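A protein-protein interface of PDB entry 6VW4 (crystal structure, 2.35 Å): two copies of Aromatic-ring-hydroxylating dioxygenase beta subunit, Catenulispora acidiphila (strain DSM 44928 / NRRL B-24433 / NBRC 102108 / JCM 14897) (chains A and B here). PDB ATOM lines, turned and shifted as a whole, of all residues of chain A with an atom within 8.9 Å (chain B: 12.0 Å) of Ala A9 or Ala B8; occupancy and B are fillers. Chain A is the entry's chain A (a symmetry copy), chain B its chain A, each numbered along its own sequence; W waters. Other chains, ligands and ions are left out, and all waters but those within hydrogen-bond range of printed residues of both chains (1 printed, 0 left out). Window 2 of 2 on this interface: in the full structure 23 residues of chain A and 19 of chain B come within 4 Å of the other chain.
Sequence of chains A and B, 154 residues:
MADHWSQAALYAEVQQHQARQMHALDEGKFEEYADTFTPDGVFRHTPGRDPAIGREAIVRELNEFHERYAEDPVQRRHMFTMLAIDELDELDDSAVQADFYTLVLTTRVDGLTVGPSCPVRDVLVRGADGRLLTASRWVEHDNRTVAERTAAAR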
ATOM      1  N   GLN A   7      -7.702 -11.161  20.772  1.00  0.00           N
ATOM      2  CA  GLN A   7      -8.842 -11.815  21.454  1.00  0.00           C
ATOM      3  C   GLN A   7     -10.219 -11.246  21.035  1.00  0.00           C
ATOM      4  O   GLN A   7     -11.220 -11.960  20.965  1.00  0.00           O
ATOM      5  CB  GLN A   7      -8.657 -11.693  22.958  1.00  0.00           C
ATOM      6  CG  GLN A   7      -8.217 -10.278  23.407  1.00  0.00           C
ATOM      7  CD  GLN A   7      -6.832  -9.807  22.905  1.00  0.00           C
ATOM      8  OE1 GLN A   7      -5.891 -10.603  22.739  1.00  0.00           O
ATOM      9  NE2 GLN A   7      -6.726  -8.495  22.645  1.00  0.00           N
ATOM     10  N   ALA A   8     -10.247  -9.958  20.715  1.00  0.00           N
ATOM     11  CA  ALA A   8     -11.431  -9.378  20.112  1.00  0.00           C
ATOM     12  C   ALA A   8     -11.803 -10.067  18.813  1.00  0.00           C
ATOM     13  O   ALA A   8     -12.992 -10.213  18.499  1.00  0.00           O
ATOM     14  CB  ALA A   8     -11.205  -7.899  19.848  1.00  0.00           C
ATOM     15  N   ALA A   9     -10.808 -10.428  18.000  1.00  0.00           N
ATOM     16  CA  ALA A   9     -11.142 -10.960  16.684  1.00  0.00           C
ATOM     17  C   ALA A   9     -11.706 -12.364  16.811  1.00  0.00           C
ATOM     18  O   ALA A   9     -12.598 -12.752  16.051  1.00  0.00           O
ATOM     19  CB  ALA A   9      -9.920 -10.967  15.765  1.00  0.00           C
ATOM     20  N   LEU A  10     -11.196 -13.138  17.771  1.00  0.00           N
ATOM     21  CA  LEU A  10     -11.769 -14.449  18.035  1.00  0.00           C
ATOM     22  C   LEU A  10     -13.203 -14.334  18.546  1.00  0.00           C
ATOM     23  O   LEU A  10     -14.039 -15.192  18.256  1.00  0.00           O
ATOM     24  CB  LEU A  10     -10.894 -15.188  19.041  1.00  0.00           C
ATOM     25  CG  LEU A  10     -11.292 -16.624  19.372  1.00  0.00           C
ATOM     26  CD1 LEU A  10     -11.257 -17.554  18.221  1.00  0.00           C
ATOM     27  CD2 LEU A  10     -10.345 -17.020  20.466  1.00  0.00           C
ATOM     28  N   TYR A  11     -13.500 -13.289  19.314  1.00  0.00           N
ATOM     29  CA  TYR A  11     -14.845 -13.130  19.863  1.00  0.00           C
ATOM     30  C   TYR A  11     -15.858 -12.984  18.732  1.00  0.00           C
ATOM     31  O   TYR A  11     -16.863 -13.706  18.669  1.00  0.00           O
ATOM     32  CB  TYR A  11     -14.846 -11.917  20.812  1.00  0.00           C
ATOM     33  CG  TYR A  11     -16.067 -11.748  21.640  1.00  0.00           C
ATOM     34  CD1 TYR A  11     -17.145 -10.991  21.174  1.00  0.00           C
ATOM     35  CD2 TYR A  11     -16.158 -12.329  22.878  1.00  0.00           C
ATOM     36  CE1 TYR A  11     -18.272 -10.832  21.928  1.00  0.00           C
ATOM     37  CE2 TYR A  11     -17.274 -12.166  23.648  1.00  0.00           C
ATOM     38  CZ  TYR A  11     -18.333 -11.433  23.164  1.00  0.00           C
ATOM     39  OH  TYR A  11     -19.426 -11.291  23.950  1.00  0.00           O
ATOM     40  N   ALA A  12     -15.567 -12.104  17.785  1.00  0.00           N
ATOM     41  CA  ALA A  12     -16.410 -11.974  16.594  1.00  0.00           C
ATOM     42  C   ALA A  12     -16.444 -13.255  15.757  1.00  0.00           C
ATOM     43  O   ALA A  12     -17.486 -13.605  15.177  1.00  0.00           O
ATOM     44  CB  ALA A  12     -15.925 -10.800  15.737  1.00  0.00           C
ATOM     45  N   GLU A  13     -15.313 -13.941  15.635  1.00  0.00           N
ATOM     46  CA  GLU A  13     -15.301 -15.183  14.867  1.00  0.00           C
ATOM     47  C   GLU A  13     -16.203 -16.247  15.505  1.00  0.00           C
ATOM     48  O   GLU A  13     -16.894 -16.986  14.797  1.00  0.00           O
ATOM     49  CB  GLU A  13     -13.861 -15.689  14.749  1.00  0.00           C
ATOM     50  CG  GLU A  13     -13.602 -16.536  13.516  1.00  0.00           C
ATOM     51  CD  GLU A  13     -12.237 -17.235  13.505  1.00  0.00           C
ATOM     52  OE1 GLU A  13     -11.323 -16.866  14.274  1.00  0.00           O
ATOM     53  OE2 GLU A  13     -12.105 -18.190  12.712  1.00  0.00           O
ATOM     54  N   VAL A  14     -16.210 -16.351  16.841  1.00  0.00           N
ATOM     55  CA  VAL A  14     -17.111 -17.316  17.494  1.00  0.00           C
ATOM     56  C   VAL A  14     -18.580 -16.948  17.243  1.00  0.00           C
ATOM     57  O   VAL A  14     -19.407 -17.813  16.905  1.00  0.00           O
ATOM     58  CB  VAL A  14     -16.822 -17.426  18.996  1.00  0.00           C
ATOM     59  CG1 VAL A  14     -17.939 -18.298  19.671  1.00  0.00           C
ATOM     60  CG2 VAL A  14     -15.424 -18.001  19.237  1.00  0.00           C
ATOM     61  N   GLN A  15     -18.918 -15.662  17.366  1.00  0.00           N
ATOM     62  CA  GLN A  15     -20.295 -15.245  17.104  1.00  0.00           C
ATOM     63  C   GLN A  15     -20.708 -15.564  15.669  1.00  0.00           C
ATOM     64  O   GLN A  15     -21.831 -16.026  15.428  1.00  0.00           O
ATOM     65  CB  GLN A  15     -20.458 -13.755  17.352  1.00  0.00           C
ATOM     66  CG  GLN A  15     -20.160 -13.301  18.722  1.00  0.00           C
ATOM     67  CD  GLN A  15     -20.137 -11.776  18.798  1.00  0.00           C
ATOM     68  OE1 GLN A  15     -19.159 -11.110  18.397  1.00  0.00           O
ATOM     69  NE2 GLN A  15     -21.216 -11.215  19.279  1.00  0.00           N
ATOM     70  N   GLN A  16     -19.804 -15.325  14.701  1.00  0.00           N
ATOM     71  CA  GLN A  16     -20.114 -15.607  13.302  1.00  0.00           C
ATOM     72  C   GLN A  16     -20.350 -17.093  13.094  1.00  0.00           C
ATOM     73  O   GLN A  16     -21.274 -17.498  12.365  1.00  0.00           O
ATOM     74  CB  GLN A  16     -18.978 -15.116  12.398  1.00  0.00           C
ATOM     75  CG  GLN A  16     -19.028 -15.646  10.957  1.00  0.00           C
ATOM     76  CD  GLN A  16     -19.738 -14.680   9.987  1.00  0.00           C
ATOM     77  OE1 GLN A  16     -20.253 -13.642  10.397  1.00  0.00           O
ATOM     78  NE2 GLN A  16     -19.769 -15.031   8.703  1.00  0.00           N
ATOM     79  N   ILE A  85     -15.756 -15.703  26.368  1.00  0.00           N
ATOM     80  CA  ILE A  85     -14.814 -16.714  25.897  1.00  0.00           C
ATOM     81  C   ILE A  85     -13.616 -16.769  26.851  1.00  0.00           C
ATOM     82  O   ILE A  85     -13.315 -15.814  27.584  1.00  0.00           O
ATOM     83  CB  ILE A  85     -14.340 -16.463  24.452  1.00  0.00           C
ATOM     84  CG1 ILE A  85     -13.602 -15.127  24.390  1.00  0.00           C
ATOM     85  CG2 ILE A  85     -15.481 -16.546  23.459  1.00  0.00           C
ATOM     86  CD1 ILE A  85     -13.025 -14.812  22.992  1.00  0.00           C
ATOM     87  N   ARG A 126      -9.745 -25.151  16.096  1.00  0.00           N
ATOM     88  CA  ARG A 126      -9.508 -24.729  14.727  1.00  0.00           C
ATOM     89  C   ARG A 126      -9.179 -25.950  13.881  1.00  0.00           C
ATOM     90  O   ARG A 126      -8.402 -26.811  14.296  1.00  0.00           O
ATOM     91  CB  ARG A 126      -8.387 -23.697  14.682  1.00  0.00           C
ATOM     92  CG  ARG A 126      -8.663 -22.643  13.681  1.00  0.00           C
ATOM     93  CD  ARG A 126      -7.679 -21.538  13.828  1.00  0.00           C
ATOM     94  NE  ARG A 126      -8.112 -20.490  14.743  1.00  0.00           N
ATOM     95  CZ  ARG A 126      -9.077 -19.623  14.479  1.00  0.00           C
ATOM     96  NH1 ARG A 126      -9.736 -19.712  13.334  1.00  0.00           N
ATOM     97  NH2 ARG A 126      -9.396 -18.685  15.382  1.00  0.00           N
ATOM     98  N   LEU A 132     -13.084 -22.504  12.296  1.00  0.00           N
ATOM     99  CA  LEU A 132     -13.465 -22.992  13.617  1.00  0.00           C
ATOM    100  C   LEU A 132     -14.405 -24.179  13.476  1.00  0.00           C
ATOM    101  O   LEU A 132     -15.205 -24.261  12.534  1.00  0.00           O
ATOM    102  CB  LEU A 132     -14.179 -21.902  14.433  1.00  0.00           C
ATOM    103  CG  LEU A 132     -13.357 -20.758  15.038  1.00  0.00           C
ATOM    104  CD1 LEU A 132     -14.318 -19.727  15.672  1.00  0.00           C
ATOM    105  CD2 LEU A 132     -12.363 -21.282  16.049  1.00  0.00           C
ATOM    106  N   GLN B   7     -11.930  -8.664   9.017  1.00  0.00           N
ATOM    107  CA  GLN B   7     -13.350  -9.082   8.977  1.00  0.00           C
ATOM    108  C   GLN B   7     -14.044  -9.039  10.360  1.00  0.00           C
ATOM    109  O   GLN B   7     -15.234  -8.743  10.478  1.00  0.00           O
ATOM    110  CB  GLN B   7     -13.439 -10.480   8.386  1.00  0.00           C
ATOM    111  CG  GLN B   7     -12.379 -11.454   8.957  1.00  0.00           C
ATOM    112  CD  GLN B   7     -10.903 -11.104   8.653  1.00  0.00           C
ATOM    113  OE1 GLN B   7     -10.567 -10.552   7.590  1.00  0.00           O
ATOM    114  NE2 GLN B   7     -10.024 -11.416   9.617  1.00  0.00           N
ATOM    115  N   ALA B   8     -13.273  -9.297  11.409  1.00  0.00           N
ATOM    116  CA  ALA B   8     -13.769  -9.078  12.754  1.00  0.00           C
ATOM    117  C   ALA B   8     -14.192  -7.638  12.978  1.00  0.00           C
ATOM    118  O   ALA B   8     -15.161  -7.375  13.702  1.00  0.00           O
ATOM    119  CB  ALA B   8     -12.699  -9.449  13.766  1.00  0.00           C
ATOM    120  N   ALA B   9     -13.436  -6.683  12.434  1.00  0.00           N
ATOM    121  CA  ALA B   9     -13.735  -5.292  12.753  1.00  0.00           C
ATOM    122  C   ALA B   9     -15.006  -4.852  12.047  1.00  0.00           C
ATOM    123  O   ALA B   9     -15.784  -4.063  12.590  1.00  0.00           O
ATOM    124  CB  ALA B   9     -12.576  -4.374  12.365  1.00  0.00           C
ATOM    125  N   LEU B  10     -15.231  -5.357  10.832  1.00  0.00           N
ATOM    126  CA  LEU B  10     -16.483  -5.082  10.146  1.00  0.00           C
ATOM    127  C   LEU B  10     -17.669  -5.690  10.891  1.00  0.00           C
ATOM    128  O   LEU B  10     -18.764  -5.123  10.891  1.00  0.00           O
ATOM    129  CB  LEU B  10     -16.406  -5.618   8.722  1.00  0.00           C
ATOM    130  CG  LEU B  10     -17.604  -5.337   7.816  1.00  0.00           C
ATOM    131  CD1 LEU B  10     -17.867  -3.901   7.571  1.00  0.00           C
ATOM    132  CD2 LEU B  10     -17.293  -6.093   6.559  1.00  0.00           C
ATOM    133  N   TYR B  11     -17.472  -6.847  11.519  1.00  0.00           N
ATOM    134  CA  TYR B  11     -18.569  -7.502  12.227  1.00  0.00           C
ATOM    135  C   TYR B  11     -19.067  -6.612  13.361  1.00  0.00           C
ATOM    136  O   TYR B  11     -20.265  -6.320  13.473  1.00  0.00           O
ATOM    137  CB  TYR B  11     -18.078  -8.873  12.730  1.00  0.00           C
ATOM    138  CG  TYR B  11     -19.126  -9.777  13.266  1.00  0.00           C
ATOM    139  CD1 TYR B  11     -19.465  -9.750  14.621  1.00  0.00           C
ATOM    140  CD2 TYR B  11     -19.779 -10.656  12.443  1.00  0.00           C
ATOM    141  CE1 TYR B  11     -20.430 -10.576  15.122  1.00  0.00           C
ATOM    142  CE2 TYR B  11     -20.736 -11.498  12.934  1.00  0.00           C
ATOM    143  CZ  TYR B  11     -21.069 -11.443  14.268  1.00  0.00           C
ATOM    144  OH  TYR B  11     -22.023 -12.289  14.724  1.00  0.00           O
ATOM    145  N   ALA B  12     -18.143  -6.108  14.168  1.00  0.00           N
ATOM    146  CA  ALA B  12     -18.502  -5.145  15.213  1.00  0.00           C
ATOM    147  C   ALA B  12     -19.083  -3.850  14.641  1.00  0.00           C
ATOM    148  O   ALA B  12     -19.996  -3.250  15.233  1.00  0.00           O
ATOM    149  CB  ALA B  12     -17.276  -4.833  16.077  1.00  0.00           C
ATOM    150  N   GLU B  13     -18.542  -3.371  13.526  1.00  0.00           N
ATOM    151  CA  GLU B  13     -19.078  -2.151  12.927  1.00  0.00           C
ATOM    152  C   GLU B  13     -20.530  -2.340  12.472  1.00  0.00           C
ATOM    153  O   GLU B  13     -21.357  -1.436  12.628  1.00  0.00           O
ATOM    154  CB  GLU B  13     -18.188  -1.732  11.754  1.00  0.00           C
ATOM    155  CG  GLU B  13     -18.210  -0.242  11.464  1.00  0.00           C
ATOM    156  CD  GLU B  13     -17.512   0.157  10.159  1.00  0.00           C
ATOM    157  OE1 GLU B  13     -16.728  -0.630   9.585  1.00  0.00           O
ATOM    158  OE2 GLU B  13     -17.784   1.287   9.702  1.00  0.00           O
ATOM    159  N   VAL B  14     -20.866  -3.505  11.899  1.00  0.00           N
ATOM    160  CA  VAL B  14     -22.265  -3.749  11.507  1.00  0.00           C
ATOM    161  C   VAL B  14     -23.180  -3.779  12.739  1.00  0.00           C
ATOM    162  O   VAL B  14     -24.262  -3.165  12.747  1.00  0.00           O
ATOM    163  CB  VAL B  14     -22.402  -5.040  10.691  1.00  0.00           C
ATOM    164  CG1 VAL B  14     -23.925  -5.358  10.485  1.00  0.00           C
ATOM    165  CG2 VAL B  14     -21.658  -4.918   9.359  1.00  0.00           C
ATOM    166  N   GLN B  15     -22.749  -4.457  13.805  1.00  0.00           N
ATOM    167  CA  GLN B  15     -23.560  -4.491  15.021  1.00  0.00           C
ATOM    168  C   GLN B  15     -23.779  -3.088  15.582  1.00  0.00           C
ATOM    169  O   GLN B  15     -24.889  -2.752  16.016  1.00  0.00           O
ATOM    170  CB  GLN B  15     -22.899  -5.356  16.081  1.00  0.00           C
ATOM    171  CG  GLN B  15     -22.683  -6.765  15.708  1.00  0.00           C
ATOM    172  CD  GLN B  15     -21.818  -7.477  16.746  1.00  0.00           C
ATOM    173  OE1 GLN B  15     -20.578  -7.329  16.786  1.00  0.00           O
ATOM    174  NE2 GLN B  15     -22.462  -8.223  17.606  1.00  0.00           N
ATOM    175  N   GLN B  16     -22.725  -2.252  15.578  1.00  0.00           N
ATOM    176  CA  GLN B  16     -22.847  -0.890  16.090  1.00  0.00           C
ATOM    177  C   GLN B  16     -23.833  -0.090  15.256  1.00  0.00           C
ATOM    178  O   GLN B  16     -24.653   0.676  15.796  1.00  0.00           O
ATOM    179  CB  GLN B  16     -21.477  -0.202  16.100  1.00  0.00           C
ATOM    180  CG  GLN B  16     -21.524   1.321  16.297  1.00  0.00           C
ATOM    181  CD  GLN B  16     -21.348   1.740  17.771  1.00  0.00           C
ATOM    182  OE1 GLN B  16     -21.257   0.895  18.659  1.00  0.00           O
ATOM    183  NE2 GLN B  16     -21.310   3.046  18.025  1.00  0.00           N
ATOM    184  N   HIS B  17     -23.721  -0.214  13.933  1.00  0.00           N
ATOM    185  CA  HIS B  17     -24.616   0.485  13.018  1.00  0.00           C
ATOM    186  C   HIS B  17     -26.048  -0.001  13.205  1.00  0.00           C
ATOM    187  O   HIS B  17     -26.978   0.796  13.283  1.00  0.00           O
ATOM    188  CB  HIS B  17     -24.120   0.240  11.572  1.00  0.00           C
ATOM    189  CG  HIS B  17     -25.042   0.732  10.502  1.00  0.00           C
ATOM    190  ND1 HIS B  17     -25.150   2.068  10.162  1.00  0.00           N
ATOM    191  CD2 HIS B  17     -25.877   0.057   9.667  1.00  0.00           C
ATOM    192  CE1 HIS B  17     -26.041   2.193   9.192  1.00  0.00           C
ATOM    193  NE2 HIS B  17     -26.477   0.988   8.856  1.00  0.00           N
ATOM    194  N   GLN B  18     -26.255  -1.319  13.295  1.00  0.00           N
ATOM    195  CA  GLN B  18     -27.631  -1.793  13.490  1.00  0.00           C
ATOM    196  C   GLN B  18     -28.202  -1.307  14.812  1.00  0.00           C
ATOM    197  O   GLN B  18     -29.364  -0.896  14.879  1.00  0.00           O
ATOM    198  CB  GLN B  18     -27.694  -3.311  13.398  1.00  0.00           C
ATOM    199  CG  GLN B  18     -27.467  -3.799  11.960  1.00  0.00           C
ATOM    200  CD  GLN B  18     -27.359  -5.279  11.888  1.00  0.00           C
ATOM    201  OE1 GLN B  18     -26.966  -5.914  12.863  1.00  0.00           O
ATOM    202  NE2 GLN B  18     -27.706  -5.852  10.733  1.00  0.00           N
ATOM    203  N   LEU B  83     -25.910 -12.743  14.064  1.00  0.00           N
ATOM    204  CA  LEU B  83     -25.461 -12.043  12.865  1.00  0.00           C
ATOM    205  C   LEU B  83     -24.403 -12.878  12.142  1.00  0.00           C
ATOM    206  O   LEU B  83     -23.428 -13.315  12.761  1.00  0.00           O
ATOM    207  CB  LEU B  83     -24.874 -10.668  13.195  1.00  0.00           C
ATOM    208  CG  LEU B  83     -24.155  -9.894  12.056  1.00  0.00           C
ATOM    209  CD1 LEU B  83     -25.212  -9.466  11.046  1.00  0.00           C
ATOM    210  CD2 LEU B  83     -23.440  -8.658  12.603  1.00  0.00           C
ATOM    211  N   ALA B  84     -24.588 -13.103  10.836  1.00  0.00           N
ATOM    212  CA  ALA B  84     -23.528 -13.651   9.981  1.00  0.00           C
ATOM    213  C   ALA B  84     -23.318 -12.721   8.787  1.00  0.00           C
ATOM    214  O   ALA B  84     -24.289 -12.266   8.179  1.00  0.00           O
ATOM    215  CB  ALA B  84     -23.866 -15.075   9.514  1.00  0.00           C
ATOM    216  N   ILE B  85     -22.075 -12.356   8.497  1.00  0.00           N
ATOM    217  CA  ILE B  85     -21.797 -11.439   7.396  1.00  0.00           C
ATOM    218  C   ILE B  85     -21.065 -12.195   6.283  1.00  0.00           C
ATOM    219  O   ILE B  85     -20.433 -13.240   6.504  1.00  0.00           O
ATOM    220  CB  ILE B  85     -20.983 -10.206   7.836  1.00  0.00           C
ATOM    221  CG1 ILE B  85     -19.625 -10.664   8.364  1.00  0.00           C
ATOM    222  CG2 ILE B  85     -21.740  -9.352   8.832  1.00  0.00           C
ATOM    223  CD1 ILE B  85     -18.701  -9.494   8.771  1.00  0.00           C
ATOM    224  N   ASP B  86     -21.185 -11.670   5.060  1.00  0.00           N
ATOM    225  CA  ASP B  86     -20.508 -12.223   3.882  1.00  0.00           C
ATOM    226  C   ASP B  86     -20.200 -11.114   2.870  1.00  0.00           C
ATOM    227  O   ASP B  86     -20.957 -10.140   2.727  1.00  0.00           O
ATOM    228  CB  ASP B  86     -21.352 -13.321   3.221  1.00  0.00           C
ATOM    229  N   GLU B  87     -19.078 -11.260   2.168  1.00  0.00           N
ATOM    230  CA  GLU B  87     -18.752 -10.337   1.071  1.00  0.00           C
ATOM    231  C   GLU B  87     -19.323 -10.815  -0.268  1.00  0.00           C
ATOM    232  O   GLU B  87     -20.224 -10.174  -0.828  1.00  0.00           O
ATOM    233  CB  GLU B  87     -17.251 -10.160   0.949  1.00  0.00           C
ATOM    234  N   VAL B  96     -21.579  -5.390   1.767  1.00  0.00           N
ATOM    235  CA  VAL B  96     -21.606  -6.533   2.673  1.00  0.00           C
ATOM    236  C   VAL B  96     -23.036  -6.961   2.938  1.00  0.00           C
ATOM    237  O   VAL B  96     -23.927  -6.134   3.162  1.00  0.00           O
ATOM    238  CB  VAL B  96     -20.875  -6.240   3.997  1.00  0.00           C
ATOM    239  CG1 VAL B  96     -21.564  -5.162   4.760  1.00  0.00           C
ATOM    240  CG2 VAL B  96     -20.765  -7.517   4.830  1.00  0.00           C
ATOM    241  N   ARG B 126     -20.521   1.333   2.087  1.00  0.00           N
ATOM    242  CA  ARG B 126     -19.815   2.408   2.761  1.00  0.00           C
ATOM    243  C   ARG B 126     -20.069   3.712   2.018  1.00  0.00           C
ATOM    244  O   ARG B 126     -20.019   3.754   0.788  1.00  0.00           O
ATOM    245  CB  ARG B 126     -18.326   2.091   2.840  1.00  0.00           C
ATOM    246  CG  ARG B 126     -17.747   2.531   4.128  1.00  0.00           C
ATOM    247  CD  ARG B 126     -16.365   1.998   4.269  1.00  0.00           C
ATOM    248  NE  ARG B 126     -16.305   0.698   4.925  1.00  0.00           N
ATOM    249  CZ  ARG B 126     -16.533   0.504   6.214  1.00  0.00           C
ATOM    250  NH1 ARG B 126     -16.877   1.532   6.976  1.00  0.00           N
ATOM    251  NH2 ARG B 126     -16.441  -0.730   6.729  1.00  0.00           N
ATOM    252  N   LEU B 132     -20.921   3.419   7.387  1.00  0.00           N
ATOM    253  CA  LEU B 132     -21.770   2.405   6.771  1.00  0.00           C
ATOM    254  C   LEU B 132     -23.164   2.969   6.545  1.00  0.00           C
ATOM    255  O   LEU B 132     -23.658   3.800   7.318  1.00  0.00           O
ATOM    256  CB  LEU B 132     -21.891   1.158   7.662  1.00  0.00           C
ATOM    257  CG  LEU B 132     -20.710   0.184   7.753  1.00  0.00           C
ATOM    258  CD1 LEU B 132     -21.024  -0.891   8.819  1.00  0.00           C
ATOM    259  CD2 LEU B 132     -20.417  -0.440   6.409  1.00  0.00           C
HETATM  260  O   HOH W   1     -18.836  -8.468  18.446  1.00  0.00           O
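Gln A7 touches none of the printed residues of chain B.
No residue of chain B comes within 4 Å of Ala A8.
Ala A9 touches just one residue of chain B: Ala B8 (3.6 Å).
No residue of chain B comes within 4 Å of Leu A10.
Of the printed residues of chain B, Ala A12 touches Tyr B11.
No residue of chain B comes within 4 Å of Glu A13.
Leu A132 touches none of the printed residues of chain B.
No residue of chain A comes within 4 Å of Gln B7.
No residue of chain A comes within 4 Å of Ala B9.
Printed residues of chain A within 4 Å of Tyr B11: Ala A12, Gln A15 and Gln A16.
Glu B13 touches none of the printed residues of chain A.
Printed residues of chain A within 4 Å of Gln B15: Gln A15.
Of the printed residues of chain A, Leu B83 touches Gln A16 (3.97 Å).
Printed residues of chain A within 4 Å of Ile B85: Gln A16 (2.9 Å).
The nearest residue of chain B that does not touch Ala A9 is Gln B7 (6.2 Å).
The nearest printed residue of chain A that does not touch Ala B8 is Ala A12 (4.01 Å).
The nearest printed residue of chain A that does not touch Leu B83 is Gln A15 (4.1 Å).
Ala A9 touches Ala B8, but with the chains exchanged Ala A8 does not touch Ala B9 (7.0 Å).
Gln A15 touches Tyr B11, but with the chains exchanged Tyr A11 does not touch Gln B15 (6.6 Å).
Gln A15 touches its own counterpart, Gln B15.
Gln A16 touches Tyr B11, but with the chains exchanged Tyr A11 does not touch Gln B16 (11.6 Å).
13 positions are printed for both chains.
O of Ile B85 sits at hydrogen-bond distance from NE2 of Gln A16.
OH of Tyr B11 lies within hydrogen-bond range of O of Leu B83 (2.6 Å).
O of Tyr A11 lies close to OE1 of Gln A15 (3.5 Å).
O of Tyr B11 lies close to OE1 of Gln B15, 3.5 Å away.
Of the 20 printed residues of chain B, 6 touch a printed residue of chain A.
Printed residues of chain A that touch a printed residue of chain B: Ala A9, Ala A12, Gln A15 and Gln A16.
Hydrophobic or aromatic side chains of chain A within 4 Å of the printed part of chain B: Ala A9 and Ala A12.
Along chain A the printed residues that touch a printed residue of chain B span positions 9 to 16.
Among the printed residues, no Asp or Glu carboxylate lies within 4 Å of a Lys or Arg side-chain nitrogen of the other chain.
Among the printed residues, pairs that only touch across the chains: Ala A9 with Ala B8, Ala A12 with Tyr B11, Gln A15 with Tyr B11, Gln A15 with Gln B15, Gln A16 with Tyr B11, Gln A16 with Leu B83 and Gln A16 with Ala B84.
Water W1 lies within hydrogen-bond range of OE1 of Gln B15 and OE1 of Gln A15.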
